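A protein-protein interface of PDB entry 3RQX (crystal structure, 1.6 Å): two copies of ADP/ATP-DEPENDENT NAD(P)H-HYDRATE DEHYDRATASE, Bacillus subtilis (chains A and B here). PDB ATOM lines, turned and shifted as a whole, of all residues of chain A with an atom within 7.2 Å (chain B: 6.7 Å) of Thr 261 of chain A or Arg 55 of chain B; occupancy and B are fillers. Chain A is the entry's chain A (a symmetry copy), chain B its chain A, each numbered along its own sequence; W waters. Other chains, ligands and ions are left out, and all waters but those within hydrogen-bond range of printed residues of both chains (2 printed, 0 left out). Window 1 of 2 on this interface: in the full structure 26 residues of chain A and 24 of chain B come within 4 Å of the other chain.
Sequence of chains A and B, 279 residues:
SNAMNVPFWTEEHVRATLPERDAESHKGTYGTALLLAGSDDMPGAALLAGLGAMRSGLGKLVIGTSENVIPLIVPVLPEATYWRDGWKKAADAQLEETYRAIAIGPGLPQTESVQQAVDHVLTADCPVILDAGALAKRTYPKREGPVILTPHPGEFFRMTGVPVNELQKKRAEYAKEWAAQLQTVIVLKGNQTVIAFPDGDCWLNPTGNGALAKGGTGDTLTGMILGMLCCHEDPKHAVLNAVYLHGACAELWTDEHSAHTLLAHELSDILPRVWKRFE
No position is printed for both chains. Of the 23 pairs that touch across the chains among the printed residues, none has its exchanged pair printed and touching as well.
Arg 55 of chain B touches Trp 253 of chain A. Trp 253 of chain A touches Pro 272 of chain B (CZ2 to CB, 3.6 Å). CA of His 257 of chain A touches O of Pro 272 of chain B (3.4 Å). CD of Lys 276 of chain B touches O of His 257 of chain A, at 3.8 Å. OG of Ser 258 of chain A touches CD1 of Trp 275 of chain B, 3.5 Å away. O of Ala 259 of chain A touches CD of Arg 21 of chain B (3.3 Å). His 260 of chain A touches Arg 55 of chain B (O to O, 3.5 Å). CG2 of Thr 261 of chain A touches CE3 of Trp 275 of chain B, 3.5 Å away. CD2 of Leu 263 of chain A touches CB of Met 54 of chain B, 3.7 Å away. Leu 263 of chain A touches Arg 55 of chain B (CG to NH1, 3.7 Å).
NH1 of Arg 21 of chain B lies within hydrogen-bond range of ND1 of His 260 of chain A, 2.9 Å away. The backbone carbonyl oxygen (O) of Met 54 of chain B is in hydrogen-bond range of the side-chain amino group (NZ) of Lys 214 of chain A (2.7 Å). The backbone carbonyl oxygen (O) of Thr 261 of chain A sits at hydrogen-bond distance from the guanidinium group (NH1) of Arg 55 of chain B, 2.8 Å away. The guanidinium group of Arg 55 of chain B lies within salt-bridge range of the side-chain carboxylate of Glu 266 of chain A. The backbone carbonyl oxygen (O) of His 260 of chain A is in hydrogen-bond range of the backbone NH (N) of Gly 57 of chain B (3.1 Å). The backbone carbonyl oxygen (O) of Pro 272 of chain B sits at hydrogen-bond distance from the backbone NH (N) of Ser 258 of chain A (3.0 Å). The side-chain carboxylate (OE1) of Glu 279 of chain B is in hydrogen-bond range of the side-chain hydroxyl (OG) of Ser 258 of chain A, at 2.7 Å.
Water W2 bridges the side-chain carboxylate (OE2) of Glu 279 of chain B (2.7 Å) and the backbone NH (N) of Ala 259 of chain A (2.8 Å). Water W1 lies within hydrogen-bond range of NE of Arg 273 of chain B and NE2 of His 257 of chain A.
NH2 of Arg 21 of chain B is in hydrogen-bond range of O of Leu 58 of chain B, at 3.0 Å. The guanidinium group (NE) of Arg 55 of chain B lies within hydrogen-bond range of the backbone carbonyl oxygen (O) of Ser 268 of chain B, at 3.0 Å. O of His 260 of chain A sits at hydrogen-bond distance from NZ of Lys 214 of chain A (2.8 Å). A ring nitrogen (ND1) of His 257 of chain A lies within hydrogen-bond range of the backbone carbonyl oxygen (O) of Trp 253 of chain A (2.8 Å). O of Ser 258 of chain A is in hydrogen-bond range of OG1 of Thr 261 of chain A (2.8 Å). The backbone NH (N) of Leu 263 of chain A is in hydrogen-bond range of the side-chain carboxylate (OE1) of Glu 266 of chain A, 3.0 Å away.
Hydrophobic or aromatic side chains of chain A within 4 Å of the printed part of chain B: Trp 253, His 257, His 260 and Leu 263. Of the 24 printed residues of chain B, 10 touch a printed residue of chain A.
Printed residues of chain B within 4 Å of Trp 253 of chain A: Arg 55 (3.7 Å) and Pro 272 (3.6 Å). Of chain B, only Arg 55 (2.8 Å), Pro 272 (3.2 Å) and Trp 275 (3.5 Å) come within 4 Å of Thr 261 of chain A. Of the printed residues of chain A, Met 54 of chain B touches Lys 214 (2.7 Å) and Leu 263 (3.7 Å). Arg 55 of chain B touches just these residues of chain A: Trp 253, His 260, Thr 261, Leu 263 and Glu 266. The nearest residue of chain B that does not touch Thr 261 of chain A is Leu 271 of chain B (4.6 Å). The nearest printed residue of chain B that does not touch Lys 214 of chain A is Arg 21 of chain B (4.04 Å).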
ATOM      1  N   ALA A 211      24.456  -4.360  24.643  1.00  0.00           N
ATOM      2  CA  ALA A 211      25.190  -5.393  25.422  1.00  0.00           C
ATOM      3  C   ALA A 211      26.165  -4.750  26.369  1.00  0.00           C
ATOM      4  O   ALA A 211      26.523  -5.341  27.403  1.00  0.00           O
ATOM      5  CB  ALA A 211      25.933  -6.390  24.489  1.00  0.00           C
ATOM      6  N   LYS A 214      25.907  -2.567  31.051  1.00  0.00           N
ATOM      7  CA  LYS A 214      26.006  -3.481  32.199  1.00  0.00           C
ATOM      8  C   LYS A 214      27.286  -3.166  32.937  1.00  0.00           C
ATOM      9  O   LYS A 214      28.300  -2.778  32.326  1.00  0.00           O
ATOM     10  CB  LYS A 214      25.941  -4.961  31.753  1.00  0.00           C
ATOM     11  CG  LYS A 214      25.716  -5.965  32.883  1.00  0.00           C
ATOM     12  CD  LYS A 214      25.727  -7.424  32.426  1.00  0.00           C
ATOM     13  CE  LYS A 214      24.544  -7.762  31.493  1.00  0.00           C
ATOM     14  NZ  LYS A 214      24.787  -9.142  30.916  1.00  0.00           N
ATOM     15  N   TRP A 253      30.049  -9.940  19.593  1.00  0.00           N
ATOM     16  CA  TRP A 253      29.296 -10.744  20.544  1.00  0.00           C
ATOM     17  C   TRP A 253      27.856 -10.963  20.100  1.00  0.00           C
ATOM     18  O   TRP A 253      27.358 -12.101  20.151  1.00  0.00           O
ATOM     19  CB  TRP A 253      29.251 -10.073  21.915  1.00  0.00           C
ATOM     20  CG  TRP A 253      28.388 -10.769  22.964  1.00  0.00           C
ATOM     21  CD1 TRP A 253      27.136 -10.411  23.367  1.00  0.00           C
ATOM     22  CD2 TRP A 253      28.753 -11.881  23.733  1.00  0.00           C
ATOM     23  NE1 TRP A 253      26.692 -11.243  24.336  1.00  0.00           N
ATOM     24  CE2 TRP A 253      27.677 -12.151  24.612  1.00  0.00           C
ATOM     25  CE3 TRP A 253      29.905 -12.657  23.822  1.00  0.00           C
ATOM     26  CZ2 TRP A 253      27.715 -13.171  25.526  1.00  0.00           C
ATOM     27  CZ3 TRP A 253      29.937 -13.699  24.698  1.00  0.00           C
ATOM     28  CH2 TRP A 253      28.837 -13.953  25.564  1.00  0.00           C
ATOM     29  N   HIS A 257      25.223 -14.273  20.113  1.00  0.00           N
ATOM     30  CA  HIS A 257      24.850 -14.266  21.534  1.00  0.00           C
ATOM     31  C   HIS A 257      23.868 -13.138  21.805  1.00  0.00           C
ATOM     32  O   HIS A 257      23.942 -12.058  21.216  1.00  0.00           O
ATOM     33  CB  HIS A 257      26.076 -14.054  22.411  1.00  0.00           C
ATOM     34  CG  HIS A 257      27.249 -14.940  22.080  1.00  0.00           C
ATOM     35  ND1 HIS A 257      28.180 -14.634  21.105  1.00  0.00           N
ATOM     36  CD2 HIS A 257      27.636 -16.133  22.606  1.00  0.00           C
ATOM     37  CE1 HIS A 257      29.089 -15.600  21.057  1.00  0.00           C
ATOM     38  NE2 HIS A 257      28.792 -16.517  21.959  1.00  0.00           N
ATOM     39  N   SER A 258      22.963 -13.344  22.762  1.00  0.00           N
ATOM     40  CA  SER A 258      22.012 -12.272  23.111  1.00  0.00           C
ATOM     41  C   SER A 258      22.721 -11.094  23.768  1.00  0.00           C
ATOM     42  O   SER A 258      23.609 -11.249  24.635  1.00  0.00           O
ATOM     43  CB  SER A 258      20.954 -12.800  24.087  1.00  0.00           C
ATOM     44  OG  SER A 258      20.229 -11.692  24.611  1.00  0.00           O
ATOM     45  N   ALA A 259      22.321  -9.894  23.353  1.00  0.00           N
ATOM     46  CA  ALA A 259      22.799  -8.665  23.942  1.00  0.00           C
ATOM     47  C   ALA A 259      22.533  -8.575  25.446  1.00  0.00           C
ATOM     48  O   ALA A 259      23.229  -7.822  26.152  1.00  0.00           O
ATOM     49  CB  ALA A 259      22.169  -7.487  23.242  1.00  0.00           C
ATOM     50  N   HIS A 260      21.610  -9.355  25.985  1.00  0.00           N
ATOM     51  CA  HIS A 260      21.364  -9.307  27.433  1.00  0.00           C
ATOM     52  C   HIS A 260      22.441  -9.984  28.253  1.00  0.00           C
ATOM     53  O   HIS A 260      22.451  -9.843  29.463  1.00  0.00           O
ATOM     54  CB  HIS A 260      20.046  -9.972  27.764  1.00  0.00           C
ATOM     55  CG  HIS A 260      18.863  -9.194  27.285  1.00  0.00           C
ATOM     56  ND1 HIS A 260      18.532  -7.964  27.812  1.00  0.00           N
ATOM     57  CD2 HIS A 260      17.971  -9.458  26.307  1.00  0.00           C
ATOM     58  CE1 HIS A 260      17.439  -7.525  27.188  1.00  0.00           C
ATOM     59  NE2 HIS A 260      17.073  -8.413  26.284  1.00  0.00           N
ATOM     60  N   THR A 261      23.294 -10.773  27.605  1.00  0.00           N
ATOM     61  CA  THR A 261      24.081 -11.813  28.306  1.00  0.00           C
ATOM     62  C   THR A 261      25.587 -11.589  28.352  1.00  0.00           C
ATOM     63  O   THR A 261      26.283 -12.410  28.881  1.00  0.00           O
ATOM     64  CB  THR A 261      23.813 -13.192  27.668  1.00  0.00           C
ATOM     65  OG1 THR A 261      24.399 -13.255  26.351  1.00  0.00           O
ATOM     66  CG2 THR A 261      22.310 -13.467  27.602  1.00  0.00           C
ATOM     67  N   LEU A 262      26.115 -10.500  27.800  1.00  0.00           N
ATOM     68  CA  LEU A 262      27.521 -10.221  27.758  1.00  0.00           C
ATOM     69  C   LEU A 262      28.048  -9.902  29.138  1.00  0.00           C
ATOM     70  O   LEU A 262      27.425  -9.177  29.900  1.00  0.00           O
ATOM     71  CB  LEU A 262      27.841  -9.048  26.843  1.00  0.00           C
ATOM     72  CG  LEU A 262      29.289  -8.580  26.725  1.00  0.00           C
ATOM     73  CD1 LEU A 262      30.238  -9.623  26.089  1.00  0.00           C
ATOM     74  CD2 LEU A 262      29.363  -7.228  25.987  1.00  0.00           C
ATOM     75  N   LEU A 263      29.202 -10.455  29.482  1.00  0.00           N
ATOM     76  CA  LEU A 263      29.955  -9.993  30.664  1.00  0.00           C
ATOM     77  C   LEU A 263      31.189  -9.203  30.199  1.00  0.00           C
ATOM     78  O   LEU A 263      31.859  -9.600  29.268  1.00  0.00           O
ATOM     79  CB  LEU A 263      30.392 -11.155  31.545  1.00  0.00           C
ATOM     80  CG  LEU A 263      29.243 -12.067  31.983  1.00  0.00           C
ATOM     81  CD1 LEU A 263      29.784 -13.307  32.663  1.00  0.00           C
ATOM     82  CD2 LEU A 263      28.331 -11.283  32.942  1.00  0.00           C
ATOM     83  N   ALA A 264      31.458  -8.073  30.860  1.00  0.00           N
ATOM     84  CA  ALA A 264      32.513  -7.171  30.444  1.00  0.00           C
ATOM     85  C   ALA A 264      33.835  -7.841  30.126  1.00  0.00           C
ATOM     86  O   ALA A 264      34.504  -7.458  29.158  1.00  0.00           O
ATOM     87  CB  ALA A 264      32.736  -6.072  31.534  1.00  0.00           C
ATOM     88  N   HIS A 265      34.283  -8.747  30.984  1.00  0.00           N
ATOM     89  CA  HIS A 265      35.612  -9.354  30.742  1.00  0.00           C
ATOM     90  C   HIS A 265      35.691 -10.030  29.394  1.00  0.00           C
ATOM     91  O   HIS A 265      36.779 -10.191  28.863  1.00  0.00           O
ATOM     92  CB  HIS A 265      36.032 -10.295  31.867  1.00  0.00           C
ATOM     93  CG  HIS A 265      35.265 -11.571  31.953  1.00  0.00           C
ATOM     94  ND1 HIS A 265      34.134 -11.714  32.719  1.00  0.00           N
ATOM     95  CD2 HIS A 265      35.485 -12.776  31.357  1.00  0.00           C
ATOM     96  CE1 HIS A 265      33.706 -12.975  32.616  1.00  0.00           C
ATOM     97  NE2 HIS A 265      34.491 -13.623  31.779  1.00  0.00           N
ATOM     98  N   GLU A 266      34.547 -10.502  28.842  1.00  0.00           N
ATOM     99  CA  GLU A 266      34.547 -11.172  27.579  1.00  0.00           C
ATOM    100  C   GLU A 266      34.939 -10.192  26.462  1.00  0.00           C
ATOM    101  O   GLU A 266      35.427 -10.609  25.404  1.00  0.00           O
ATOM    102  CB  GLU A 266      33.195 -11.825  27.319  1.00  0.00           C
ATOM    103  CG  GLU A 266      32.968 -12.963  28.254  1.00  0.00           C
ATOM    104  CD  GLU A 266      31.600 -13.567  28.215  1.00  0.00           C
ATOM    105  OE1 GLU A 266      30.591 -12.818  28.261  1.00  0.00           O
ATOM    106  OE2 GLU A 266      31.549 -14.834  28.085  1.00  0.00           O
ATOM    107  N   ARG B  21      17.027  -5.275  23.995  1.00  0.00           N
ATOM    108  CA  ARG B  21      17.998  -4.377  24.599  1.00  0.00           C
ATOM    109  C   ARG B  21      18.372  -3.318  23.606  1.00  0.00           C
ATOM    110  O   ARG B  21      19.333  -3.484  22.837  1.00  0.00           O
ATOM    111  CB  ARG B  21      19.220  -5.179  25.030  1.00  0.00           C
ATOM    112  CG  ARG B  21      19.831  -4.669  26.365  1.00  0.00           C
ATOM    113  CD  ARG B  21      20.938  -5.545  26.808  1.00  0.00           C
ATOM    114  NE  ARG B  21      21.560  -5.122  28.060  1.00  0.00           N
ATOM    115  CZ  ARG B  21      21.178  -5.469  29.264  1.00  0.00           C
ATOM    116  NH1 ARG B  21      20.179  -6.265  29.440  1.00  0.00           N
ATOM    117  NH2 ARG B  21      21.834  -5.003  30.319  1.00  0.00           N
ATOM    118  N   GLY B  50      25.228 -15.587  41.200  1.00  0.00           N
ATOM    119  CA  GLY B  50      25.789 -14.360  40.643  1.00  0.00           C
ATOM    120  C   GLY B  50      25.987 -14.394  39.164  1.00  0.00           C
ATOM    121  O   GLY B  50      25.586 -13.459  38.429  1.00  0.00           O
ATOM    122  N   LEU B  51      26.567 -15.478  38.669  1.00  0.00           N
ATOM    123  CA  LEU B  51      26.780 -15.671  37.244  1.00  0.00           C
ATOM    124  C   LEU B  51      25.421 -15.721  36.531  1.00  0.00           C
ATOM    125  O   LEU B  51      25.225 -15.094  35.497  1.00  0.00           O
ATOM    126  CB  LEU B  51      27.534 -16.960  37.021  1.00  0.00           C
ATOM    127  CG  LEU B  51      28.992 -16.917  37.250  1.00  0.00           C
ATOM    128  CD1 LEU B  51      29.533 -18.375  37.432  1.00  0.00           C
ATOM    129  CD2 LEU B  51      29.803 -16.197  36.117  1.00  0.00           C
ATOM    130  N   GLY B  52      24.470 -16.503  37.074  1.00  0.00           N
ATOM    131  CA  GLY B  52      23.171 -16.577  36.409  1.00  0.00           C
ATOM    132  C   GLY B  52      22.514 -15.236  36.334  1.00  0.00           C
ATOM    133  O   GLY B  52      21.897 -14.909  35.343  1.00  0.00           O
ATOM    134  N   ALA B  53      22.642 -14.419  37.358  1.00  0.00           N
ATOM    135  CA  ALA B  53      22.006 -13.100  37.380  1.00  0.00           C
ATOM    136  C   ALA B  53      22.653 -12.151  36.389  1.00  0.00           C
ATOM    137  O   ALA B  53      21.962 -11.511  35.592  1.00  0.00           O
ATOM    138  CB  ALA B  53      22.034 -12.511  38.833  1.00  0.00           C
ATOM    139  N   MET B  54      23.988 -12.051  36.393  1.00  0.00           N
ATOM    140  CA  MET B  54      24.656 -11.138  35.450  1.00  0.00           C
ATOM    141  C   MET B  54      24.526 -11.545  34.005  1.00  0.00           C
ATOM    142  O   MET B  54      24.505 -10.683  33.121  1.00  0.00           O
ATOM    143  CB  MET B  54      26.098 -10.879  35.893  1.00  0.00           C
ATOM    144  CG  MET B  54      26.185 -10.289  37.281  1.00  0.00           C
ATOM    145  SD  MET B  54      27.628  -9.194  37.484  1.00  0.00           S
ATOM    146  CE  MET B  54      27.058  -7.785  36.570  1.00  0.00           C
ATOM    147  N   ARG B  55      24.402 -12.853  33.754  1.00  0.00           N
ATOM    148  CA  ARG B  55      24.112 -13.357  32.447  1.00  0.00           C
ATOM    149  C   ARG B  55      22.711 -12.994  31.960  1.00  0.00           C
ATOM    150  O   ARG B  55      22.450 -13.139  30.756  1.00  0.00           O
ATOM    151  CB  ARG B  55      24.287 -14.890  32.406  1.00  0.00           C
ATOM    152  CG  ARG B  55      25.722 -15.309  32.313  1.00  0.00           C
ATOM    153  CD  ARG B  55      26.254 -15.041  30.913  1.00  0.00           C
ATOM    154  NE  ARG B  55      27.540 -15.773  30.704  1.00  0.00           N
ATOM    155  CZ  ARG B  55      28.493 -15.388  29.880  1.00  0.00           C
ATOM    156  NH1 ARG B  55      28.382 -14.283  29.180  1.00  0.00           N
ATOM    157  NH2 ARG B  55      29.604 -16.093  29.784  1.00  0.00           N
ATOM    158  N   SER B  56      21.800 -12.615  32.836  1.00  0.00           N
ATOM    159  CA  SER B  56      20.386 -12.600  32.512  1.00  0.00           C
ATOM    160  C   SER B  56      19.803 -11.194  32.397  1.00  0.00           C
ATOM    161  O   SER B  56      18.636 -10.984  32.710  1.00  0.00           O
ATOM    162  CB  SER B  56      19.603 -13.510  33.472  1.00  0.00           C
ATOM    163  OG  SER B  56      19.996 -14.851  33.284  1.00  0.00           O
ATOM    164  N   GLY B  57      20.594 -10.215  31.954  1.00  0.00           N
ATOM    165  CA  GLY B  57      20.017  -8.972  31.474  1.00  0.00           C
ATOM    166  C   GLY B  57      19.837  -7.806  32.447  1.00  0.00           C
ATOM    167  O   GLY B  57      19.231  -6.814  32.067  1.00  0.00           O
ATOM    168  N   LEU B  58      20.347  -7.966  33.663  1.00  0.00           N
ATOM    169  CA  LEU B  58      20.374  -6.885  34.627  1.00  0.00           C
ATOM    170  C   LEU B  58      21.360  -5.798  34.176  1.00  0.00           C
ATOM    171  O   LEU B  58      22.066  -5.934  33.183  1.00  0.00           O
ATOM    172  CB  LEU B  58      20.628  -7.364  36.020  1.00  0.00           C
ATOM    173  CG  LEU B  58      21.843  -8.229  36.297  1.00  0.00           C
ATOM    174  CD1 LEU B  58      23.160  -7.462  35.971  1.00  0.00           C
ATOM    175  CD2 LEU B  58      21.856  -8.672  37.732  1.00  0.00           C
ATOM    176  N   LEU B  77      33.746 -13.556  38.273  1.00  0.00           N
ATOM    177  CA  LEU B  77      32.662 -12.613  37.979  1.00  0.00           C
ATOM    178  C   LEU B  77      33.126 -11.243  38.450  1.00  0.00           C
ATOM    179  O   LEU B  77      32.596 -10.691  39.443  1.00  0.00           O
ATOM    180  CB  LEU B  77      31.394 -13.060  38.708  1.00  0.00           C
ATOM    181  CG  LEU B  77      30.140 -12.249  38.327  1.00  0.00           C
ATOM    182  CD1 LEU B  77      29.721 -12.353  36.858  1.00  0.00           C
ATOM    183  CD2 LEU B  77      28.998 -12.689  39.261  1.00  0.00           C
ATOM    184  N   MET B 224      19.274 -16.553  37.427  1.00  0.00           N
ATOM    185  CA  MET B 224      18.570 -16.275  36.189  1.00  0.00           C
ATOM    186  C   MET B 224      17.263 -15.526  36.376  1.00  0.00           C
ATOM    187  O   MET B 224      16.962 -14.572  35.623  1.00  0.00           O
ATOM    188  CB  MET B 224      18.431 -17.505  35.293  1.00  0.00           C
ATOM    189  CG  MET B 224      19.741 -18.046  34.852  1.00  0.00           C
ATOM    190  SD  MET B 224      19.554 -19.573  33.874  1.00  0.00           S
ATOM    191  CE  MET B 224      18.374 -19.004  32.616  1.00  0.00           C
ATOM    192  N   GLY B 227      18.028 -11.805  37.395  1.00  0.00           N
ATOM    193  CA  GLY B 227      18.376 -10.984  36.239  1.00  0.00           C
ATOM    194  C   GLY B 227      17.162 -10.749  35.334  1.00  0.00           C
ATOM    195  O   GLY B 227      16.919  -9.600  34.923  1.00  0.00           O
ATOM    196  N   MET B 228      16.356 -11.780  35.067  1.00  0.00           N
ATOM    197  CA  MET B 228      15.247 -11.569  34.156  1.00  0.00           C
ATOM    198  C   MET B 228      14.199 -10.644  34.755  1.00  0.00           C
ATOM    199  O   MET B 228      13.564  -9.885  34.026  1.00  0.00           O
ATOM    200  CB  MET B 228      14.731 -12.912  33.639  1.00  0.00           C
ATOM    201  CG  MET B 228      15.701 -13.403  32.353  1.00  0.00           C
ATOM    202  SD  MET B 228      14.974 -14.930  31.838  1.00  0.00           S
ATOM    203  CE  MET B 228      16.477 -15.684  31.269  1.00  0.00           C
ATOM    204  N   LEU B 267      25.610 -23.866  32.606  1.00  0.00           N
ATOM    205  CA  LEU B 267      24.324 -23.391  32.121  1.00  0.00           C
ATOM    206  C   LEU B 267      24.414 -21.893  31.788  1.00  0.00           C
ATOM    207  O   LEU B 267      23.883 -21.477  30.750  1.00  0.00           O
ATOM    208  CB  LEU B 267      23.227 -23.630  33.141  1.00  0.00           C
ATOM    209  CG  LEU B 267      22.871 -25.094  33.358  1.00  0.00           C
ATOM    210  CD1 LEU B 267      22.131 -25.173  34.741  1.00  0.00           C
ATOM    211  CD2 LEU B 267      22.039 -25.709  32.231  1.00  0.00           C
ATOM    212  N   SER B 268      25.069 -21.121  32.635  1.00  0.00           N
ATOM    213  CA  SER B 268      25.264 -19.697  32.404  1.00  0.00           C
ATOM    214  C   SER B 268      26.116 -19.384  31.202  1.00  0.00           C
ATOM    215  O   SER B 268      25.963 -18.338  30.609  1.00  0.00           O
ATOM    216  CB  SER B 268      25.925 -19.025  33.603  1.00  0.00           C
ATOM    217  OG  SER B 268      25.231 -19.286  34.751  1.00  0.00           O
ATOM    218  N   ASP B 269      27.095 -20.243  30.951  1.00  0.00           N
ATOM    219  CA  ASP B 269      28.024 -20.104  29.802  1.00  0.00           C
ATOM    220  C   ASP B 269      27.248 -20.394  28.499  1.00  0.00           C
ATOM    221  O   ASP B 269      27.631 -19.894  27.412  1.00  0.00           O
ATOM    222  CB  ASP B 269      29.211 -21.148  29.744  1.00  0.00           C
ATOM    223  CG  ASP B 269      30.248 -21.221  30.947  1.00  0.00           C
ATOM    224  OD1 ASP B 269      30.552 -20.238  31.658  1.00  0.00           O
ATOM    225  OD2 ASP B 269      30.891 -22.339  31.118  1.00  0.00           O
ATOM    226  N   ILE B 270      26.204 -21.257  28.553  1.00  0.00           N
ATOM    227  CA  ILE B 270      25.406 -21.713  27.375  1.00  0.00           C
ATOM    228  C   ILE B 270      24.303 -20.719  27.060  1.00  0.00           C
ATOM    229  O   ILE B 270      23.922 -20.556  25.902  1.00  0.00           O
ATOM    230  CB  ILE B 270      24.802 -23.168  27.644  1.00  0.00           C
ATOM    231  CG1 ILE B 270      25.959 -24.174  27.724  1.00  0.00           C
ATOM    232  CG2 ILE B 270      23.677 -23.555  26.662  1.00  0.00           C
ATOM    233  CD1 ILE B 270      25.530 -25.495  28.326  1.00  0.00           C
ATOM    234  N   LEU B 271      23.783 -20.082  28.098  1.00  0.00           N
ATOM    235  CA  LEU B 271      22.671 -19.152  27.982  1.00  0.00           C
ATOM    236  C   LEU B 271      22.855 -18.100  26.887  1.00  0.00           C
ATOM    237  O   LEU B 271      21.890 -17.829  26.187  1.00  0.00           O
ATOM    238  CB  LEU B 271      22.337 -18.535  29.365  1.00  0.00           C
ATOM    239  CG  LEU B 271      21.149 -17.575  29.375  1.00  0.00           C
ATOM    240  CD1 LEU B 271      19.809 -18.273  28.979  1.00  0.00           C
ATOM    241  CD2 LEU B 271      21.049 -16.853  30.716  1.00  0.00           C
ATOM    242  N   PRO B 272      24.061 -17.491  26.732  1.00  0.00           N
ATOM    243  CA  PRO B 272      24.192 -16.466  25.667  1.00  0.00           C
ATOM    244  C   PRO B 272      23.736 -16.953  24.292  1.00  0.00           C
ATOM    245  O   PRO B 272      23.043 -16.237  23.556  1.00  0.00           O
ATOM    246  CB  PRO B 272      25.681 -16.154  25.659  1.00  0.00           C
ATOM    247  CG  PRO B 272      26.068 -16.344  27.150  1.00  0.00           C
ATOM    248  CD  PRO B 272      25.280 -17.580  27.543  1.00  0.00           C
ATOM    249  N   ARG B 273      24.153 -18.150  23.899  1.00  0.00           N
ATOM    250  CA  ARG B 273      23.781 -18.657  22.577  1.00  0.00           C
ATOM    251  C   ARG B 273      22.330 -19.136  22.521  1.00  0.00           C
ATOM    252  O   ARG B 273      21.674 -18.975  21.484  1.00  0.00           O
ATOM    253  CB  ARG B 273      24.721 -19.799  22.170  1.00  0.00           C
ATOM    254  CG  ARG B 273      26.065 -19.337  21.744  1.00  0.00           C
ATOM    255  CD  ARG B 273      26.941 -20.531  21.279  1.00  0.00           C
ATOM    256  NE  ARG B 273      28.246 -20.001  20.873  1.00  0.00           N
ATOM    257  CZ  ARG B 273      28.540 -19.560  19.654  1.00  0.00           C
ATOM    258  NH1 ARG B 273      27.645 -19.592  18.688  1.00  0.00           N
ATOM    259  NH2 ARG B 273      29.749 -19.063  19.415  1.00  0.00           N
ATOM    260  N   TRP B 275      19.748 -18.056  24.356  1.00  0.00           N
ATOM    261  CA  TRP B 275      18.890 -16.874  24.369  1.00  0.00           C
ATOM    262  C   TRP B 275      18.823 -16.274  22.948  1.00  0.00           C
ATOM    263  O   TRP B 275      17.741 -15.896  22.493  1.00  0.00           O
ATOM    264  CB  TRP B 275      19.355 -15.889  25.431  1.00  0.00           C
ATOM    265  CG  TRP B 275      18.439 -14.722  25.765  1.00  0.00           C
ATOM    266  CD1 TRP B 275      17.563 -14.012  24.945  1.00  0.00           C
ATOM    267  CD2 TRP B 275      18.347 -14.123  27.064  1.00  0.00           C
ATOM    268  NE1 TRP B 275      16.967 -13.017  25.684  1.00  0.00           N
ATOM    269  CE2 TRP B 275      17.434 -13.070  26.978  1.00  0.00           C
ATOM    270  CE3 TRP B 275      18.988 -14.367  28.284  1.00  0.00           C
ATOM    271  CZ2 TRP B 275      17.136 -12.261  28.051  1.00  0.00           C
ATOM    272  CZ3 TRP B 275      18.675 -13.565  29.355  1.00  0.00           C
ATOM    273  CH2 TRP B 275      17.751 -12.538  29.247  1.00  0.00           C
ATOM    274  N   LYS B 276      19.942 -16.161  22.247  1.00  0.00           N
ATOM    275  CA  LYS B 276      19.971 -15.614  20.887  1.00  0.00           C
ATOM    276  C   LYS B 276      18.955 -16.317  19.978  1.00  0.00           C
ATOM    277  O   LYS B 276      18.336 -15.684  19.126  1.00  0.00           O
ATOM    278  CB  LYS B 276      21.367 -15.747  20.316  1.00  0.00           C
ATOM    279  CG  LYS B 276      21.560 -15.199  18.887  1.00  0.00           C
ATOM    280  CD  LYS B 276      21.387 -13.662  18.863  1.00  0.00           C
ATOM    281  CE  LYS B 276      21.618 -13.134  17.470  1.00  0.00           C
ATOM    282  NZ  LYS B 276      21.602 -11.656  17.457  1.00  0.00           N
ATOM    283  N   GLU B 279      15.381 -14.969  20.004  1.00  0.00           N
ATOM    284  CA  GLU B 279      15.245 -13.557  19.685  1.00  0.00           C
ATOM    285  C   GLU B 279      14.773 -13.330  18.248  1.00  0.00           C
ATOM    286  O   GLU B 279      14.720 -14.262  17.468  1.00  0.00           O
ATOM    287  CB  GLU B 279      16.572 -12.815  19.950  1.00  0.00           C
ATOM    288  CG  GLU B 279      16.892 -12.700  21.436  1.00  0.00           C
ATOM    289  CD  GLU B 279      18.112 -11.830  21.753  1.00  0.00           C
ATOM    290  OE1 GLU B 279      18.154 -11.257  22.881  1.00  0.00           O
ATOM    291  OE2 GLU B 279      18.998 -11.721  20.885  1.00  0.00           O
ATOM    292  OXT GLU B 279      14.443 -12.207  17.863  1.00  0.00           O
HETATM  293  O   HOH W   1      29.372 -19.052  23.147  1.00  0.00           O
HETATM  294  O   HOH W   2      20.671  -9.632  21.081  1.00  0.00           O
